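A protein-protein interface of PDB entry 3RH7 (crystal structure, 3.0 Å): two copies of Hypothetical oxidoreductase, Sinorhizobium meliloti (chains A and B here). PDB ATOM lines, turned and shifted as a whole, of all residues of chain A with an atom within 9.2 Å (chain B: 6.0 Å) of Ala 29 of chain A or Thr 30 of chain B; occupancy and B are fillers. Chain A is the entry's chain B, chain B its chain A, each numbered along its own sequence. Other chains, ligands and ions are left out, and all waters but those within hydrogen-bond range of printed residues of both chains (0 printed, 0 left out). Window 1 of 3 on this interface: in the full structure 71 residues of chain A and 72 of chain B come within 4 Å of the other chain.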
ATOM      1  N   ASP A  23      15.344  27.212  -3.640  1.00  0.00           N
ATOM      2  CA  ASP A  23      15.174  26.712  -2.267  1.00  0.00           C
ATOM      3  C   ASP A  23      13.721  26.275  -2.029  1.00  0.00           C
ATOM      4  O   ASP A  23      13.517  25.213  -1.420  1.00  0.00           O
ATOM      5  CB  ASP A  23      15.662  27.747  -1.226  1.00  0.00           C
ATOM      6  CG  ASP A  23      17.193  27.936  -1.163  1.00  0.00           C
ATOM      7  OD1 ASP A  23      17.926  27.143  -1.829  1.00  0.00           O
ATOM      8  OD2 ASP A  23      17.662  28.874  -0.442  1.00  0.00           O
ATOM      9  N   ALA A  24      12.734  27.022  -2.613  1.00  0.00           N
ATOM     10  CA  ALA A  24      11.300  26.698  -2.520  1.00  0.00           C
ATOM     11  C   ALA A  24      10.991  25.393  -3.244  1.00  0.00           C
ATOM     12  O   ALA A  24      10.290  24.545  -2.691  1.00  0.00           O
ATOM     13  CB  ALA A  24      10.463  27.823  -3.077  1.00  0.00           C
ATOM     14  N   PHE A  25      11.574  25.185  -4.436  1.00  0.00           N
ATOM     15  CA  PHE A  25      11.398  23.946  -5.192  1.00  0.00           C
ATOM     16  C   PHE A  25      11.960  22.770  -4.420  1.00  0.00           C
ATOM     17  O   PHE A  25      11.378  21.679  -4.447  1.00  0.00           O
ATOM     18  CB  PHE A  25      12.070  24.039  -6.567  1.00  0.00           C
ATOM     19  CG  PHE A  25      11.405  24.929  -7.602  1.00  0.00           C
ATOM     20  CD1 PHE A  25      10.012  25.037  -7.668  1.00  0.00           C
ATOM     21  CD2 PHE A  25      12.155  25.539  -8.597  1.00  0.00           C
ATOM     22  CE1 PHE A  25       9.394  25.809  -8.656  1.00  0.00           C
ATOM     23  CE2 PHE A  25      11.528  26.287  -9.603  1.00  0.00           C
ATOM     24  CZ  PHE A  25      10.153  26.424  -9.616  1.00  0.00           C
ATOM     25  N   GLY A  26      13.059  23.017  -3.705  1.00  0.00           N
ATOM     26  CA  GLY A  26      13.767  22.028  -2.892  1.00  0.00           C
ATOM     27  C   GLY A  26      12.977  21.412  -1.756  1.00  0.00           C
ATOM     28  O   GLY A  26      13.341  20.338  -1.263  1.00  0.00           O
ATOM     29  N   ALA A  27      11.887  22.081  -1.350  1.00  0.00           N
ATOM     30  CA  ALA A  27      10.985  21.628  -0.293  1.00  0.00           C
ATOM     31  C   ALA A  27      10.326  20.279  -0.654  1.00  0.00           C
ATOM     32  O   ALA A  27      10.040  19.446   0.231  1.00  0.00           O
ATOM     33  CB  ALA A  27       9.920  22.687  -0.041  1.00  0.00           C
ATOM     34  N   PHE A  28      10.117  20.068  -1.965  1.00  0.00           N
ATOM     35  CA  PHE A  28       9.539  18.849  -2.505  1.00  0.00           C
ATOM     36  C   PHE A  28      10.641  17.825  -2.676  1.00  0.00           C
ATOM     37  O   PHE A  28      11.542  18.006  -3.509  1.00  0.00           O
ATOM     38  CB  PHE A  28       8.813  19.121  -3.822  1.00  0.00           C
ATOM     39  CG  PHE A  28       8.105  17.934  -4.408  1.00  0.00           C
ATOM     40  CD1 PHE A  28       6.800  17.633  -4.042  1.00  0.00           C
ATOM     41  CD2 PHE A  28       8.717  17.157  -5.387  1.00  0.00           C
ATOM     42  CE1 PHE A  28       6.114  16.583  -4.663  1.00  0.00           C
ATOM     43  CE2 PHE A  28       8.042  16.108  -6.001  1.00  0.00           C
ATOM     44  CZ  PHE A  28       6.747  15.819  -5.640  1.00  0.00           C
ATOM     45  N   ALA A  29      10.590  16.757  -1.834  1.00  0.00           N
ATOM     46  CA  ALA A  29      11.567  15.674  -1.898  1.00  0.00           C
ATOM     47  C   ALA A  29      11.443  14.922  -3.222  1.00  0.00           C
ATOM     48  O   ALA A  29      10.402  14.976  -3.882  1.00  0.00           O
ATOM     49  CB  ALA A  29      11.376  14.724  -0.741  1.00  0.00           C
ATOM     50  N   THR A  30      12.532  14.267  -3.639  1.00  0.00           N
ATOM     51  CA  THR A  30      12.591  13.438  -4.838  1.00  0.00           C
ATOM     52  C   THR A  30      13.489  12.265  -4.592  1.00  0.00           C
ATOM     53  O   THR A  30      14.169  12.218  -3.570  1.00  0.00           O
ATOM     54  CB  THR A  30      13.154  14.210  -6.061  1.00  0.00           C
ATOM     55  OG1 THR A  30      14.514  14.613  -5.839  1.00  0.00           O
ATOM     56  CG2 THR A  30      12.256  15.333  -6.560  1.00  0.00           C
ATOM     57  N   GLY A  31      13.548  11.378  -5.585  1.00  0.00           N
ATOM     58  CA  GLY A  31      14.515  10.300  -5.693  1.00  0.00           C
ATOM     59  C   GLY A  31      15.672  10.860  -6.514  1.00  0.00           C
ATOM     60  O   GLY A  31      15.757  12.076  -6.753  1.00  0.00           O
ATOM     61  N   VAL A  32      16.573   9.991  -6.981  1.00  0.00           N
ATOM     62  CA  VAL A  32      17.702  10.483  -7.771  1.00  0.00           C
ATOM     63  C   VAL A  32      17.874   9.553  -8.977  1.00  0.00           C
ATOM     64  O   VAL A  32      18.209   8.374  -8.824  1.00  0.00           O
ATOM     65  CB  VAL A  32      19.000  10.622  -6.905  1.00  0.00           C
ATOM     66  CG1 VAL A  32      20.244  10.824  -7.767  1.00  0.00           C
ATOM     67  CG2 VAL A  32      18.875  11.735  -5.864  1.00  0.00           C
ATOM     68  N   ASN A  50      16.859  14.873 -11.154  1.00  0.00           N
ATOM     69  CA  ASN A  50      15.926  14.558 -10.070  1.00  0.00           C
ATOM     70  C   ASN A  50      14.530  15.138 -10.408  1.00  0.00           C
ATOM     71  O   ASN A  50      13.536  14.872  -9.719  1.00  0.00           O
ATOM     72  CB  ASN A  50      16.484  15.055  -8.729  1.00  0.00           C
ATOM     73  CG  ASN A  50      16.198  16.503  -8.363  1.00  0.00           C
ATOM     74  OD1 ASN A  50      16.188  17.437  -9.200  1.00  0.00           O
ATOM     75  ND2 ASN A  50      16.002  16.726  -7.066  1.00  0.00           N
ATOM     76  N   SER A  51      14.479  15.909 -11.509  1.00  0.00           N
ATOM     77  CA  SER A  51      13.263  16.527 -12.046  1.00  0.00           C
ATOM     78  C   SER A  51      12.634  15.544 -13.019  1.00  0.00           C
ATOM     79  O   SER A  51      12.579  15.780 -14.227  1.00  0.00           O
ATOM     80  CB  SER A  51      13.587  17.864 -12.712  1.00  0.00           C
ATOM     81  OG  SER A  51      14.566  17.722 -13.735  1.00  0.00           O
ATOM     82  N   PHE A  52      12.232  14.401 -12.463  1.00  0.00           N
ATOM     83  CA  PHE A  52      11.641  13.237 -13.087  1.00  0.00           C
ATOM     84  C   PHE A  52      10.219  13.011 -12.577  1.00  0.00           C
ATOM     85  O   PHE A  52       9.944  13.249 -11.398  1.00  0.00           O
ATOM     86  CB  PHE A  52      12.523  12.024 -12.765  1.00  0.00           C
ATOM     87  CG  PHE A  52      11.892  10.671 -12.941  1.00  0.00           C
ATOM     88  CD1 PHE A  52      11.189  10.075 -11.906  1.00  0.00           C
ATOM     89  CD2 PHE A  52      12.002   9.986 -14.145  1.00  0.00           C
ATOM     90  CE1 PHE A  52      10.618   8.801 -12.062  1.00  0.00           C
ATOM     91  CE2 PHE A  52      11.434   8.707 -14.303  1.00  0.00           C
ATOM     92  CZ  PHE A  52      10.755   8.118 -13.260  1.00  0.00           C
ATOM     93  N   THR A  53       9.335  12.492 -13.440  1.00  0.00           N
ATOM     94  CA  THR A  53       7.945  12.213 -13.104  1.00  0.00           C
ATOM     95  C   THR A  53       7.404  11.040 -13.911  1.00  0.00           C
ATOM     96  O   THR A  53       7.672  10.938 -15.102  1.00  0.00           O
ATOM     97  CB  THR A  53       7.084  13.474 -13.356  1.00  0.00           C
ATOM     98  OG1 THR A  53       7.317  14.404 -12.318  1.00  0.00           O
ATOM     99  CG2 THR A  53       5.598  13.189 -13.377  1.00  0.00           C
ATOM    100  N   SER A  54       6.614  10.185 -13.257  1.00  0.00           N
ATOM    101  CA  SER A  54       5.855   9.100 -13.856  1.00  0.00           C
ATOM    102  C   SER A  54       4.590   9.759 -14.423  1.00  0.00           C
ATOM    103  O   SER A  54       3.820  10.371 -13.666  1.00  0.00           O
ATOM    104  CB  SER A  54       5.554   8.026 -12.809  1.00  0.00           C
ATOM    105  OG  SER A  54       4.989   8.543 -11.609  1.00  0.00           O
ATOM    106  N   VAL A  86      16.899   4.712 -11.521  1.00  0.00           N
ATOM    107  CA  VAL A  86      16.453   5.159 -10.195  1.00  0.00           C
ATOM    108  C   VAL A  86      17.456   4.575  -9.203  1.00  0.00           C
ATOM    109  O   VAL A  86      17.425   3.378  -8.917  1.00  0.00           O
ATOM    110  CB  VAL A  86      14.977   4.806  -9.864  1.00  0.00           C
ATOM    111  CG1 VAL A  86      14.646   5.174  -8.427  1.00  0.00           C
ATOM    112  CG2 VAL A  86      14.018   5.514 -10.812  1.00  0.00           C
ATOM    113  N   GLY A 158      15.484   3.614  -2.545  1.00  0.00           N
ATOM    114  CA  GLY A 158      16.139   4.609  -3.369  1.00  0.00           C
ATOM    115  C   GLY A 158      16.896   5.684  -2.639  1.00  0.00           C
ATOM    116  O   GLY A 158      16.570   6.013  -1.493  1.00  0.00           O
ATOM    117  N   LEU A 159      17.878   6.281  -3.335  1.00  0.00           N
ATOM    118  CA  LEU A 159      18.595   7.455  -2.851  1.00  0.00           C
ATOM    119  C   LEU A 159      17.631   8.624  -3.004  1.00  0.00           C
ATOM    120  O   LEU A 159      17.002   8.755  -4.073  1.00  0.00           O
ATOM    121  CB  LEU A 159      19.887   7.690  -3.672  1.00  0.00           C
ATOM    122  CG  LEU A 159      20.697   8.964  -3.378  1.00  0.00           C
ATOM    123  CD1 LEU A 159      21.568   8.783  -2.169  1.00  0.00           C
ATOM    124  CD2 LEU A 159      21.604   9.269  -4.512  1.00  0.00           C
ATOM    125  N   GLY A 160      17.476   9.401  -1.940  1.00  0.00           N
ATOM    126  CA  GLY A 160      16.589  10.552  -1.913  1.00  0.00           C
ATOM    127  C   GLY A 160      17.304  11.888  -1.778  1.00  0.00           C
ATOM    128  O   GLY A 160      18.390  11.973  -1.183  1.00  0.00           O
ATOM    129  N   TYR A 161      16.675  12.955  -2.320  1.00  0.00           N
ATOM    130  CA  TYR A 161      17.227  14.296  -2.266  1.00  0.00           C
ATOM    131  C   TYR A 161      16.157  15.284  -1.851  1.00  0.00           C
ATOM    132  O   TYR A 161      15.192  15.553  -2.579  1.00  0.00           O
ATOM    133  CB  TYR A 161      17.863  14.684  -3.605  1.00  0.00           C
ATOM    134  CG  TYR A 161      18.789  15.879  -3.552  1.00  0.00           C
ATOM    135  CD1 TYR A 161      20.096  15.749  -3.096  1.00  0.00           C
ATOM    136  CD2 TYR A 161      18.414  17.102  -4.102  1.00  0.00           C
ATOM    137  CE1 TYR A 161      20.997  16.818  -3.149  1.00  0.00           C
ATOM    138  CE2 TYR A 161      19.299  18.191  -4.128  1.00  0.00           C
ATOM    139  CZ  TYR A 161      20.588  18.048  -3.635  1.00  0.00           C
ATOM    140  OH  TYR A 161      21.498  19.096  -3.655  1.00  0.00           O
ATOM    141  N   ALA A 162      16.333  15.799  -0.642  1.00  0.00           N
ATOM    142  CA  ALA A 162      15.429  16.772  -0.050  1.00  0.00           C
ATOM    143  C   ALA A 162      16.197  17.925   0.482  1.00  0.00           C
ATOM    144  O   ALA A 162      17.185  17.772   1.245  1.00  0.00           O
ATOM    145  CB  ALA A 162      14.611  16.149   1.046  1.00  0.00           C
ATOM    146  N   ARG A 163      15.690  19.107   0.091  1.00  0.00           N
ATOM    147  CA  ARG A 163      16.250  20.404   0.404  1.00  0.00           C
ATOM    148  C   ARG A 163      17.720  20.380  -0.081  1.00  0.00           C
ATOM    149  O   ARG A 163      17.981  20.139  -1.294  1.00  0.00           O
ATOM    150  CB  ARG A 163      16.027  20.809   1.872  1.00  0.00           C
ATOM    151  CG  ARG A 163      14.506  20.811   2.230  1.00  0.00           C
ATOM    152  CD  ARG A 163      14.126  21.662   3.426  1.00  0.00           C
ATOM    153  NE  ARG A 163      13.280  22.815   3.086  1.00  0.00           N
ATOM    154  CZ  ARG A 163      11.954  22.812   3.147  1.00  0.00           C
ATOM    155  NH1 ARG A 163      11.303  21.715   3.487  1.00  0.00           N
ATOM    156  NH2 ARG A 163      11.266  23.902   2.839  1.00  0.00           N
ATOM    157  N   GLY A 164      18.670  20.597   0.805  1.00  0.00           N
ATOM    158  CA  GLY A 164      20.039  20.686   0.285  1.00  0.00           C
ATOM    159  C   GLY A 164      20.834  19.429  -0.023  1.00  0.00           C
ATOM    160  O   GLY A 164      21.932  19.531  -0.565  1.00  0.00           O
ATOM    161  N   GLY A 165      20.359  18.272   0.417  1.00  0.00           N
ATOM    162  CA  GLY A 165      21.151  17.066   0.309  1.00  0.00           C
ATOM    163  C   GLY A 165      20.391  15.775   0.292  1.00  0.00           C
ATOM    164  O   GLY A 165      19.152  15.734   0.236  1.00  0.00           O
ATOM    165  N   PHE A 167      19.106  12.070   1.553  1.00  0.00           N
ATOM    166  CA  PHE A 167      18.546  11.292   2.626  1.00  0.00           C
ATOM    167  C   PHE A 167      18.419   9.836   2.095  1.00  0.00           C
ATOM    168  O   PHE A 167      18.340   9.608   0.876  1.00  0.00           O
ATOM    169  CB  PHE A 167      17.228  11.869   3.103  1.00  0.00           C
ATOM    170  CG  PHE A 167      16.079  11.778   2.124  1.00  0.00           C
ATOM    171  CD1 PHE A 167      15.224  10.669   2.125  1.00  0.00           C
ATOM    172  CD2 PHE A 167      15.819  12.812   1.230  1.00  0.00           C
ATOM    173  CE1 PHE A 167      14.140  10.597   1.240  1.00  0.00           C
ATOM    174  CE2 PHE A 167      14.728  12.737   0.350  1.00  0.00           C
ATOM    175  CZ  PHE A 167      13.889  11.635   0.371  1.00  0.00           C
ATOM    176  N   PHE A 236      16.171  16.008   7.573  1.00  0.00           N
ATOM    177  CA  PHE A 236      16.518  14.603   7.411  1.00  0.00           C
ATOM    178  C   PHE A 236      17.919  14.361   8.025  1.00  0.00           C
ATOM    179  O   PHE A 236      18.708  15.287   8.185  1.00  0.00           O
ATOM    180  CB  PHE A 236      16.469  14.199   5.907  1.00  0.00           C
ATOM    181  CG  PHE A 236      15.097  14.032   5.265  1.00  0.00           C
ATOM    182  CD1 PHE A 236      14.431  12.797   5.297  1.00  0.00           C
ATOM    183  CD2 PHE A 236      14.481  15.095   4.598  1.00  0.00           C
ATOM    184  CE1 PHE A 236      13.150  12.649   4.729  1.00  0.00           C
ATOM    185  CE2 PHE A 236      13.204  14.942   4.019  1.00  0.00           C
ATOM    186  CZ  PHE A 236      12.538  13.729   4.111  1.00  0.00           C
ATOM    187  N   PHE B  28      10.925   5.696  -7.209  1.00  0.00           N
ATOM    188  CA  PHE B  28      11.343   7.088  -7.169  1.00  0.00           C
ATOM    189  C   PHE B  28      10.574   7.794  -6.092  1.00  0.00           C
ATOM    190  O   PHE B  28       9.362   7.985  -6.216  1.00  0.00           O
ATOM    191  CB  PHE B  28      11.148   7.760  -8.543  1.00  0.00           C
ATOM    192  CG  PHE B  28      11.602   9.206  -8.626  1.00  0.00           C
ATOM    193  CD1 PHE B  28      12.923   9.524  -8.906  1.00  0.00           C
ATOM    194  CD2 PHE B  28      10.702  10.246  -8.440  1.00  0.00           C
ATOM    195  CE1 PHE B  28      13.329  10.859  -8.995  1.00  0.00           C
ATOM    196  CE2 PHE B  28      11.108  11.582  -8.544  1.00  0.00           C
ATOM    197  CZ  PHE B  28      12.417  11.879  -8.814  1.00  0.00           C
ATOM    198  N   ALA B  29      11.265   8.162  -5.012  1.00  0.00           N
ATOM    199  CA  ALA B  29      10.614   8.866  -3.888  1.00  0.00           C
ATOM    200  C   ALA B  29      10.196  10.262  -4.329  1.00  0.00           C
ATOM    201  O   ALA B  29      10.789  10.809  -5.248  1.00  0.00           O
ATOM    202  CB  ALA B  29      11.545   8.934  -2.676  1.00  0.00           C
ATOM    203  N   THR B  30       9.098  10.768  -3.790  1.00  0.00           N
ATOM    204  CA  THR B  30       8.594  12.117  -4.076  1.00  0.00           C
ATOM    205  C   THR B  30       7.981  12.690  -2.841  1.00  0.00           C
ATOM    206  O   THR B  30       7.433  11.921  -2.063  1.00  0.00           O
ATOM    207  CB  THR B  30       7.488  12.139  -5.172  1.00  0.00           C
ATOM    208  OG1 THR B  30       6.292  11.562  -4.647  1.00  0.00           O
ATOM    209  CG2 THR B  30       7.888  11.498  -6.482  1.00  0.00           C
ATOM    210  N   GLY B  31       7.916  14.015  -2.759  1.00  0.00           N
ATOM    211  CA  GLY B  31       7.147  14.704  -1.746  1.00  0.00           C
ATOM    212  C   GLY B  31       5.666  14.566  -2.091  1.00  0.00           C
ATOM    213  O   GLY B  31       5.293  13.793  -2.990  1.00  0.00           O
ATOM    214  N   VAL B  32       4.794  15.286  -1.379  1.00  0.00           N
ATOM    215  CA  VAL B  32       3.351  15.212  -1.645  1.00  0.00           C
ATOM    216  C   VAL B  32       2.807  16.635  -1.808  1.00  0.00           C
ATOM    217  O   VAL B  32       3.090  17.515  -0.962  1.00  0.00           O
ATOM    218  CB  VAL B  32       2.570  14.432  -0.547  1.00  0.00           C
ATOM    219  CG1 VAL B  32       1.095  14.328  -0.904  1.00  0.00           C
ATOM    220  CG2 VAL B  32       3.166  13.045  -0.281  1.00  0.00           C
ATOM    221  N   ASN B  50       1.542  13.717  -6.609  1.00  0.00           N
ATOM    222  CA  ASN B  50       2.954  13.535  -6.293  1.00  0.00           C
ATOM    223  C   ASN B  50       3.759  13.494  -7.604  1.00  0.00           C
ATOM    224  O   ASN B  50       5.000  13.497  -7.596  1.00  0.00           O
ATOM    225  CB  ASN B  50       3.150  12.295  -5.434  1.00  0.00           C
ATOM    226  CG  ASN B  50       3.169  10.970  -6.149  1.00  0.00           C
ATOM    227  OD1 ASN B  50       2.442  10.733  -7.126  1.00  0.00           O
ATOM    228  ND2 ASN B  50       3.986  10.047  -5.651  1.00  0.00           N
ATOM    229  N   SER B  51       3.022  13.466  -8.736  1.00  0.00           N
ATOM    230  CA  SER B  51       3.595  13.473 -10.069  1.00  0.00           C
ATOM    231  C   SER B  51       3.724  14.935 -10.477  1.00  0.00           C
ATOM    232  O   SER B  51       2.966  15.426 -11.322  1.00  0.00           O
ATOM    233  CB  SER B  51       2.760  12.617 -11.028  1.00  0.00           C
ATOM    234  OG  SER B  51       3.044  11.228 -10.864  1.00  0.00           O
ATOM    235  N   PHE B  52       4.681  15.621  -9.776  1.00  0.00           N
ATOM    236  CA  PHE B  52       5.065  17.037  -9.821  1.00  0.00           C
ATOM    237  C   PHE B  52       6.586  17.193 -10.055  1.00  0.00           C
ATOM    238  O   PHE B  52       7.373  16.379  -9.554  1.00  0.00           O
ATOM    239  CB  PHE B  52       4.671  17.711  -8.492  1.00  0.00           C
ATOM    240  CG  PHE B  52       5.358  19.021  -8.162  1.00  0.00           C
ATOM    241  CD1 PHE B  52       6.565  19.044  -7.474  1.00  0.00           C
ATOM    242  CD2 PHE B  52       4.775  20.238  -8.497  1.00  0.00           C
ATOM    243  CE1 PHE B  52       7.182  20.264  -7.139  1.00  0.00           C
ATOM    244  CE2 PHE B  52       5.396  21.453  -8.162  1.00  0.00           C
ATOM    245  CZ  PHE B  52       6.588  21.458  -7.477  1.00  0.00           C
ATOM    246  N   VAL B  86       2.835  22.115  -1.339  1.00  0.00           N
ATOM    247  CA  VAL B  86       3.816  21.065  -0.965  1.00  0.00           C
ATOM    248  C   VAL B  86       3.576  20.803   0.552  1.00  0.00           C
ATOM    249  O   VAL B  86       3.911  21.637   1.397  1.00  0.00           O
ATOM    250  CB  VAL B  86       5.276  21.484  -1.345  1.00  0.00           C
ATOM    251  CG1 VAL B  86       6.301  20.430  -0.983  1.00  0.00           C
ATOM    252  CG2 VAL B  86       5.379  21.814  -2.823  1.00  0.00           C
ATOM    253  N   LEU B 159       6.086  16.334   3.702  1.00  0.00           N
ATOM    254  CA  LEU B 159       5.530  14.975   3.734  1.00  0.00           C
ATOM    255  C   LEU B 159       6.104  14.295   2.530  1.00  0.00           C
ATOM    256  O   LEU B 159       6.265  14.959   1.479  1.00  0.00           O
ATOM    257  CB  LEU B 159       3.983  15.001   3.691  1.00  0.00           C
ATOM    258  CG  LEU B 159       3.240  13.663   3.604  1.00  0.00           C
ATOM    259  CD1 LEU B 159       3.242  12.911   4.943  1.00  0.00           C
ATOM    260  CD2 LEU B 159       1.814  13.881   3.175  1.00  0.00           C
ATOM    261  N   GLY B 160       6.503  13.043   2.705  1.00  0.00           N
ATOM    262  CA  GLY B 160       7.063  12.256   1.614  1.00  0.00           C
ATOM    263  C   GLY B 160       6.204  11.050   1.315  1.00  0.00           C
ATOM    264  O   GLY B 160       5.410  10.647   2.148  1.00  0.00           O
ATOM    265  N   TYR B 161       6.341  10.492   0.117  1.00  0.00           N
ATOM    266  CA  TYR B 161       5.718   9.259  -0.359  1.00  0.00           C
ATOM    267  C   TYR B 161       6.743   8.463  -1.086  1.00  0.00           C
ATOM    268  O   TYR B 161       7.273   8.950  -2.086  1.00  0.00           O
ATOM    269  CB  TYR B 161       4.525   9.528  -1.305  1.00  0.00           C
ATOM    270  CG  TYR B 161       3.476   8.430  -1.329  1.00  0.00           C
ATOM    271  CD1 TYR B 161       2.569   8.280  -0.279  1.00  0.00           C
ATOM    272  CD2 TYR B 161       3.336   7.591  -2.432  1.00  0.00           C
ATOM    273  CE1 TYR B 161       1.543   7.327  -0.328  1.00  0.00           C
ATOM    274  CE2 TYR B 161       2.319   6.624  -2.487  1.00  0.00           C
ATOM    275  CZ  TYR B 161       1.409   6.510  -1.439  1.00  0.00           C
ATOM    276  OH  TYR B 161       0.403   5.562  -1.436  1.00  0.00           O
ATOM    277  N   ALA B 162       7.075   7.270  -0.592  1.00  0.00           N
ATOM    278  CA  ALA B 162       7.987   6.369  -1.322  1.00  0.00           C
ATOM    279  C   ALA B 162       7.411   5.012  -1.299  1.00  0.00           C
ATOM    280  O   ALA B 162       6.892   4.582  -0.250  1.00  0.00           O
ATOM    281  CB  ALA B 162       9.386   6.351  -0.742  1.00  0.00           C
ATOM    282  N   PHE B 167       6.551   8.744   4.374  1.00  0.00           N
ATOM    283  CA  PHE B 167       7.732   8.776   5.217  1.00  0.00           C
ATOM    284  C   PHE B 167       7.935  10.242   5.660  1.00  0.00           C
ATOM    285  O   PHE B 167       7.492  11.168   4.947  1.00  0.00           O
ATOM    286  CB  PHE B 167       8.937   8.188   4.465  1.00  0.00           C
ATOM    287  CG  PHE B 167       9.360   8.954   3.244  1.00  0.00           C
ATOM    288  CD1 PHE B 167      10.264   9.993   3.340  1.00  0.00           C
ATOM    289  CD2 PHE B 167       8.863   8.632   1.997  1.00  0.00           C
ATOM    290  CE1 PHE B 167      10.666  10.694   2.208  1.00  0.00           C
ATOM    291  CE2 PHE B 167       9.267   9.340   0.863  1.00  0.00           C
ATOM    292  CZ  PHE B 167      10.160  10.368   0.977  1.00  0.00           C
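The side-chain hydroxyl (OG) of Ser 51 of chain B lies within hydrogen-bond range of the backbone carbonyl oxygen (O) of Ser 54 of chain A, 3.0 Å away.
The backbone NH of Gly 31 of chain B is in hydrogen-bond range of the backbone carbonyl oxygen of Ala 29 of chain A (2.9 Å).
The backbone carbonyl oxygen (O) of Phe 52 of chain B lies within hydrogen-bond range of the side-chain hydroxyl (OG1) of Thr 53 of chain A (3.4 Å).
The backbone carbonyl oxygen (O) of Ala 29 of chain B lies within hydrogen-bond range of the backbone NH (N) of Gly 31 of chain A (2.8 Å).
The side-chain hydroxyl (OG1) of Thr 30 of chain B lies within hydrogen-bond range of the side-chain amide nitrogen (ND2) of Asn 50 of chain B (2.9 Å).
N of Tyr 161 of chain B sits at hydrogen-bond distance from O of Thr 30 of chain B (2.8 Å).
The backbone carbonyl oxygen (O) of Thr 30 of chain A sits at hydrogen-bond distance from the backbone NH (N) of Tyr 161 of chain A, 2.9 Å away.
The side-chain hydroxyl (OG1) of Thr 30 of chain A lies within hydrogen-bond range of the side-chain amide nitrogen (ND2) of Asn 50 of chain A (2.9 Å).
The backbone NH (N) of Val 32 of chain A lies within hydrogen-bond range of the backbone carbonyl oxygen (O) of Leu 159 of chain A (3.2 Å).
N of Phe 167 of chain A is in hydrogen-bond range of O of Gly 160 of chain A (2.8 Å).
CB of Thr 30 of chain B touches CZ of Phe 28 of chain A (3.8 Å).
Asn 50 of chain B touches Phe 28 of chain A (O to CZ, 3.5 Å).
Phe 52 of chain B touches Phe 28 of chain A (CD1 to CD2, 3.5 Å).
Val 86 of chain B touches Phe 28 of chain A (CG1 to CA, 3.9 Å).
Ala 29 of chain A touches Thr 30 of chain B.
CB of Thr 30 of chain A touches CZ of Phe 28 of chain B, 3.7 Å away.
Asn 50 of chain A touches Phe 28 of chain B.
Phe 52 of chain A touches Phe 28 of chain B.
N of Phe 28 of chain B touches CG1 of Val 86 of chain A, at 3.9 Å.
CE1 of Phe 167 of chain A touches CE1 of Phe 167 of chain B (3.6 Å).
Of chain B, only Thr 30 and Gly 31 come within 4 Å of Ala 29 of chain A.
Thr 30 of chain B touches just these residues of chain A: Phe 28 and Ala 29.
Of chain A, only Thr 30 (3.1 Å) and Gly 31 (2.8 Å) come within 4 Å of Ala 29 of chain B.
Of chain A, only Phe 28 and Ala 29 come within 4 Å of Gly 31 of chain B.
No residue of chain A comes within 4 Å of Gly 160 of chain B.
Printed residues of chain A within 4 Å of Phe 167 of chain B: Phe 167.
Printed residues of chain A within 4 Å of Val 86 of chain B: Phe 28.
Printed residues of chain B within 4 Å of Val 32 of chain A: Phe 28.
Of the printed residues of chain B, Phe 28 of chain A touches Thr 30, Gly 31, Val 32, Asn 50, Phe 52 and Val 86.
Printed residues of chain A within 4 Å of Phe 28 of chain B: Thr 30 (3.7 Å), Gly 31 (3.4 Å), Val 32 (3.9 Å), Asn 50 (3.3 Å), Phe 52 (3.4 Å) and Val 86 (3.9 Å).
The nearest residue of chain B that does not touch Ala 29 of chain A is Ala 29 of chain B (4.4 Å).
The nearest residue of chain A that does not touch Thr 30 of chain B is Thr 30 of chain A (4.3 Å).
Of the 26 printed residues of chain A, 11 touch a printed residue of chain B.
Printed residues of chain A that touch a printed residue of chain B: Phe 28, Ala 29, Thr 30, Gly 31, Val 32, Asn 50, Phe 52, Thr 53, Ser 54, Val 86 and Phe 167.
Hydrophobic or aromatic side chains of chain A within 4 Å of the printed part of chain B: Phe 28, Phe 52, Val 86 and Phe 167.
Phe 28 of chain A touches Thr 30 of chain B, and with the chains exchanged Thr 30 of chain A touches Phe 28 of chain B.
Phe 28 of chain A touches Gly 31 of chain B, and with the chains exchanged Gly 31 of chain A touches Phe 28 of chain B.
Phe 28 of chain A touches Phe 52 of chain B, and with the chains exchanged Phe 52 of chain A touches Phe 28 of chain B.
Ala 29 of chain A touches Gly 31 of chain B, and with the chains exchanged Gly 31 of chain A touches Ala 29 of chain B.
14 positions are printed for both chains.
Of the 20 pairs that touch across the chains among the printed residues, 17 have their exchanged pair printed and touching as well.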
